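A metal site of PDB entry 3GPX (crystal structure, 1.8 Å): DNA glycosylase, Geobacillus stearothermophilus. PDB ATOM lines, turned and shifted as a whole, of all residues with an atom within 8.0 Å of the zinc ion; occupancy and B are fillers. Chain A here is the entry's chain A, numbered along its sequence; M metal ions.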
ATOM      1  N   PHE A 181       8.974   0.794 -14.921  1.00  0.00           N
ATOM      2  CA  PHE A 181      10.017   1.733 -14.494  1.00  0.00           C
ATOM      3  C   PHE A 181      11.390   1.362 -15.074  1.00  0.00           C
ATOM      4  O   PHE A 181      12.091   2.211 -15.651  1.00  0.00           O
ATOM      5  CB  PHE A 181      10.131   1.813 -12.966  1.00  0.00           C
ATOM      6  CG  PHE A 181      11.315   2.625 -12.522  1.00  0.00           C
ATOM      7  CD1 PHE A 181      11.238   4.009 -12.489  1.00  0.00           C
ATOM      8  CD2 PHE A 181      12.550   1.999 -12.199  1.00  0.00           C
ATOM      9  CE1 PHE A 181      12.327   4.772 -12.121  1.00  0.00           C
ATOM     10  CE2 PHE A 181      13.649   2.769 -11.813  1.00  0.00           C
ATOM     11  CZ  PHE A 181      13.539   4.165 -11.767  1.00  0.00           C
ATOM     12  N   TYR A 223      11.907   0.143  -6.787  1.00  0.00           N
ATOM     13  CA  TYR A 223      12.156   1.461  -7.322  1.00  0.00           C
ATOM     14  C   TYR A 223      10.954   2.383  -7.205  1.00  0.00           C
ATOM     15  O   TYR A 223      11.119   3.580  -6.952  1.00  0.00           O
ATOM     16  CB  TYR A 223      12.539   1.374  -8.791  1.00  0.00           C
ATOM     17  CG  TYR A 223      13.908   0.803  -9.019  1.00  0.00           C
ATOM     18  CD1 TYR A 223      14.053  -0.488  -9.551  1.00  0.00           C
ATOM     19  CD2 TYR A 223      15.056   1.549  -8.744  1.00  0.00           C
ATOM     20  CE1 TYR A 223      15.305  -1.023  -9.790  1.00  0.00           C
ATOM     21  CE2 TYR A 223      16.319   1.025  -8.977  1.00  0.00           C
ATOM     22  CZ  TYR A 223      16.430  -0.268  -9.486  1.00  0.00           C
ATOM     23  OH  TYR A 223      17.676  -0.802  -9.733  1.00  0.00           O
ATOM     24  N   VAL A 224       9.764   1.845  -7.419  1.00  0.00           N
ATOM     25  CA  VAL A 224       8.576   2.686  -7.459  1.00  0.00           C
ATOM     26  C   VAL A 224       7.415   2.231  -6.601  1.00  0.00           C
ATOM     27  O   VAL A 224       6.691   3.065  -6.056  1.00  0.00           O
ATOM     28  CB  VAL A 224       8.081   2.976  -8.924  1.00  0.00           C
ATOM     29  CG1 VAL A 224       9.135   3.754  -9.720  1.00  0.00           C
ATOM     30  CG2 VAL A 224       7.698   1.699  -9.676  1.00  0.00           C
ATOM     31  N   PRO A 231      11.901  10.077  -3.172  1.00  0.00           N
ATOM     32  CA  PRO A 231      12.704  10.332  -4.365  1.00  0.00           C
ATOM     33  C   PRO A 231      12.950   9.059  -5.173  1.00  0.00           C
ATOM     34  O   PRO A 231      13.200   7.996  -4.614  1.00  0.00           O
ATOM     35  CB  PRO A 231      14.050  10.800  -3.792  1.00  0.00           C
ATOM     36  CG  PRO A 231      13.784  11.181  -2.407  1.00  0.00           C
ATOM     37  CD  PRO A 231      12.676  10.323  -1.930  1.00  0.00           C
ATOM     38  N   CYS A 232      12.929   9.202  -6.498  1.00  0.00           N
ATOM     39  CA  CYS A 232      13.341   8.130  -7.365  1.00  0.00           C
ATOM     40  C   CYS A 232      14.794   7.771  -7.042  1.00  0.00           C
ATOM     41  O   CYS A 232      15.646   8.647  -6.812  1.00  0.00           O
ATOM     42  CB  CYS A 232      13.206   8.573  -8.823  1.00  0.00           C
ATOM     43  SG  CYS A 232      13.882   7.403 -10.024  1.00  0.00           S
ATOM     44  N   LYS A 233      15.060   6.477  -6.984  1.00  0.00           N
ATOM     45  CA  LYS A 233      16.409   5.995  -6.657  1.00  0.00           C
ATOM     46  C   LYS A 233      17.423   6.194  -7.783  1.00  0.00           C
ATOM     47  O   LYS A 233      18.635   6.054  -7.566  1.00  0.00           O
ATOM     48  CB  LYS A 233      16.381   4.508  -6.253  1.00  0.00           C
ATOM     49  CG  LYS A 233      15.701   4.258  -4.923  1.00  0.00           C
ATOM     50  CD  LYS A 233      15.536   2.778  -4.632  1.00  0.00           C
ATOM     51  CE  LYS A 233      14.833   2.583  -3.290  1.00  0.00           C
ATOM     52  NZ  LYS A 233      14.778   1.144  -2.884  1.00  0.00           N
ATOM     53  N   ARG A 234      16.926   6.518  -8.984  1.00  0.00           N
ATOM     54  CA  ARG A 234      17.781   6.711 -10.148  1.00  0.00           C
ATOM     55  C   ARG A 234      18.012   8.193 -10.449  1.00  0.00           C
ATOM     56  O   ARG A 234      19.088   8.568 -10.905  1.00  0.00           O
ATOM     57  CB  ARG A 234      17.167   6.016 -11.375  1.00  0.00           C
ATOM     58  CG  ARG A 234      17.146   4.489 -11.289  1.00  0.00           C
ATOM     59  CD  ARG A 234      18.320   3.892 -12.047  1.00  0.00           C
ATOM     60  NE  ARG A 234      18.381   2.434 -11.970  1.00  0.00           N
ATOM     61  CZ  ARG A 234      17.754   1.597 -12.792  1.00  0.00           C
ATOM     62  NH1 ARG A 234      16.982   2.066 -13.767  1.00  0.00           N
ATOM     63  NH2 ARG A 234      17.891   0.287 -12.635  1.00  0.00           N
ATOM     64  N   CYS A 235      17.008   9.040 -10.199  1.00  0.00           N
ATOM     65  CA  CYS A 235      17.117  10.486 -10.556  1.00  0.00           C
ATOM     66  C   CYS A 235      16.694  11.483  -9.496  1.00  0.00           C
ATOM     67  O   CYS A 235      16.870  12.690  -9.702  1.00  0.00           O
ATOM     68  CB  CYS A 235      16.313  10.792 -11.840  1.00  0.00           C
ATOM     69  SG  CYS A 235      14.493  10.864 -11.597  1.00  0.00           S
ATOM     70  N   GLY A 236      16.132  10.999  -8.395  1.00  0.00           N
ATOM     71  CA  GLY A 236      15.727  11.873  -7.293  1.00  0.00           C
ATOM     72  C   GLY A 236      14.376  12.549  -7.405  1.00  0.00           C
ATOM     73  O   GLY A 236      13.913  13.180  -6.447  1.00  0.00           O
ATOM     74  N   THR A 237      13.729  12.440  -8.567  1.00  0.00           N
ATOM     75  CA  THR A 237      12.381  13.005  -8.772  1.00  0.00           C
ATOM     76  C   THR A 237      11.359  12.257  -7.908  1.00  0.00           C
ATOM     77  O   THR A 237      11.391  11.040  -7.847  1.00  0.00           O
ATOM     78  CB  THR A 237      11.962  12.893 -10.253  1.00  0.00           C
ATOM     79  OG1 THR A 237      12.880  13.632 -11.070  1.00  0.00           O
ATOM     80  CG2 THR A 237      10.540  13.415 -10.499  1.00  0.00           C
ATOM     81  N   PRO A 238      10.433  12.973  -7.241  1.00  0.00           N
ATOM     82  CA  PRO A 238       9.433  12.275  -6.434  1.00  0.00           C
ATOM     83  C   PRO A 238       8.604  11.300  -7.259  1.00  0.00           C
ATOM     84  O   PRO A 238       8.097  11.635  -8.353  1.00  0.00           O
ATOM     85  CB  PRO A 238       8.554  13.410  -5.895  1.00  0.00           C
ATOM     86  CG  PRO A 238       9.457  14.573  -5.877  1.00  0.00           C
ATOM     87  CD  PRO A 238      10.330  14.436  -7.092  1.00  0.00           C
ATOM     88  N   ILE A 239       8.489  10.089  -6.728  1.00  0.00           N
ATOM     89  CA  ILE A 239       7.644   9.068  -7.353  1.00  0.00           C
ATOM     90  C   ILE A 239       6.190   9.497  -7.236  1.00  0.00           C
ATOM     91  O   ILE A 239       5.799  10.070  -6.214  1.00  0.00           O
ATOM     92  CB  ILE A 239       7.889   7.689  -6.717  1.00  0.00           C
ATOM     93  CG1 ILE A 239       9.368   7.291  -6.933  1.00  0.00           C
ATOM     94  CG2 ILE A 239       6.874   6.624  -7.244  1.00  0.00           C
ATOM     95  CD1 ILE A 239       9.845   7.394  -8.426  1.00  0.00           C
ATOM     96  N   TYR A 251       5.069   5.485 -10.521  1.00  0.00           N
ATOM     97  CA  TYR A 251       6.009   5.733 -11.602  1.00  0.00           C
ATOM     98  C   TYR A 251       6.867   6.970 -11.345  1.00  0.00           C
ATOM     99  O   TYR A 251       6.486   7.861 -10.563  1.00  0.00           O
ATOM    100  CB  TYR A 251       5.254   5.881 -12.932  1.00  0.00           C
ATOM    101  CG  TYR A 251       4.290   7.052 -12.930  1.00  0.00           C
ATOM    102  CD1 TYR A 251       4.684   8.287 -13.455  1.00  0.00           C
ATOM    103  CD2 TYR A 251       2.993   6.930 -12.417  1.00  0.00           C
ATOM    104  CE1 TYR A 251       3.830   9.369 -13.445  1.00  0.00           C
ATOM    105  CE2 TYR A 251       2.122   8.029 -12.404  1.00  0.00           C
ATOM    106  CZ  TYR A 251       2.554   9.237 -12.923  1.00  0.00           C
ATOM    107  OH  TYR A 251       1.722  10.337 -12.925  1.00  0.00           O
ATOM    108  N   CYS A 252       8.010   7.004 -12.010  1.00  0.00           N
ATOM    109  CA  CYS A 252       8.834   8.225 -12.026  1.00  0.00           C
ATOM    110  C   CYS A 252       8.509   8.973 -13.293  1.00  0.00           C
ATOM    111  O   CYS A 252       8.722   8.468 -14.402  1.00  0.00           O
ATOM    112  CB  CYS A 252      10.338   7.872 -12.007  1.00  0.00           C
ATOM    113  SG  CYS A 252      11.336   9.379 -12.198  1.00  0.00           S
ATOM    114  N   PRO A 253       8.023  10.216 -13.145  1.00  0.00           N
ATOM    115  CA  PRO A 253       7.640  10.982 -14.319  1.00  0.00           C
ATOM    116  C   PRO A 253       8.817  11.470 -15.172  1.00  0.00           C
ATOM    117  O   PRO A 253       8.594  11.934 -16.295  1.00  0.00           O
ATOM    118  CB  PRO A 253       6.859  12.159 -13.720  1.00  0.00           C
ATOM    119  CG  PRO A 253       7.420  12.326 -12.354  1.00  0.00           C
ATOM    120  CD  PRO A 253       7.733  10.932 -11.889  1.00  0.00           C
ATOM    121  N   ARG A 254      10.048  11.340 -14.671  1.00  0.00           N
ATOM    122  CA  ARG A 254      11.244  11.682 -15.437  1.00  0.00           C
ATOM    123  C   ARG A 254      11.865  10.481 -16.163  1.00  0.00           C
ATOM    124  O   ARG A 254      12.196  10.581 -17.346  1.00  0.00           O
ATOM    125  CB  ARG A 254      12.280  12.345 -14.532  1.00  0.00           C
ATOM    126  CG  ARG A 254      13.540  12.746 -15.284  1.00  0.00           C
ATOM    127  CD  ARG A 254      14.555  13.455 -14.407  1.00  0.00           C
ATOM    128  NE  ARG A 254      15.748  13.715 -15.183  1.00  0.00           N
ATOM    129  CZ  ARG A 254      16.807  14.399 -14.770  1.00  0.00           C
ATOM    130  NH1 ARG A 254      17.830  14.605 -15.607  1.00  0.00           N
ATOM    131  NH2 ARG A 254      16.866  14.870 -13.524  1.00  0.00           N
ATOM    132  N   CYS A 255      12.017   9.362 -15.458  1.00  0.00           N
ATOM    133  CA  CYS A 255      12.688   8.154 -15.974  1.00  0.00           C
ATOM    134  C   CYS A 255      11.802   7.448 -17.014  1.00  0.00           C
ATOM    135  O   CYS A 255      12.310   6.817 -17.942  1.00  0.00           O
ATOM    136  CB  CYS A 255      13.040   7.180 -14.823  1.00  0.00           C
ATOM    137  SG  CYS A 255      14.483   7.697 -13.708  1.00  0.00           S
ATOM    138  N   GLN A 256      10.495   7.588 -16.859  1.00  0.00           N
ATOM    139  CA  GLN A 256       9.517   6.912 -17.719  1.00  0.00           C
ATOM    140  C   GLN A 256       8.841   7.850 -18.701  1.00  0.00           C
ATOM    141  O   GLN A 256       8.438   8.951 -18.325  1.00  0.00           O
ATOM    142  CB  GLN A 256       8.467   6.221 -16.851  1.00  0.00           C
ATOM    143  CG  GLN A 256       9.055   5.068 -16.062  1.00  0.00           C
ATOM    144  CD  GLN A 256       8.129   4.533 -15.035  1.00  0.00           C
ATOM    145  OE1 GLN A 256       8.286   4.804 -13.839  1.00  0.00           O
ATOM    146  NE2 GLN A 256       7.166   3.722 -15.461  1.00  0.00           N
HETATM  147 ZN    ZN M   1      13.549   8.752 -11.892  1.00  0.00          ZN
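Four residues have an atom within 4 Å of the zinc ion: Cys 232, Cys 235, Cys 252 and Cys 255.
The zinc ion is bound by the side-chain sulfur (SG) of Cys 255, the side-chain sulfur (SG) of Cys 252, the side-chain sulfur (SG) of Cys 232 and the side-chain sulfur (SG) of Cys 235.
The side-chain sulfur (SG) of Cys 252 lies close to the backbone NH (N) of Arg 254 (3.4 Å).
N of Cys 252 sits at hydrogen-bond distance from OE1 of Gln 256.
SG of Cys 232 lies close to N of Arg 234 (3.3 Å).
O of Thr 237 sits at hydrogen-bond distance from N of Cys 232 (2.8 Å).
OG1 of Thr 237 sits close to SG of Cys 235, 3.2 Å away.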
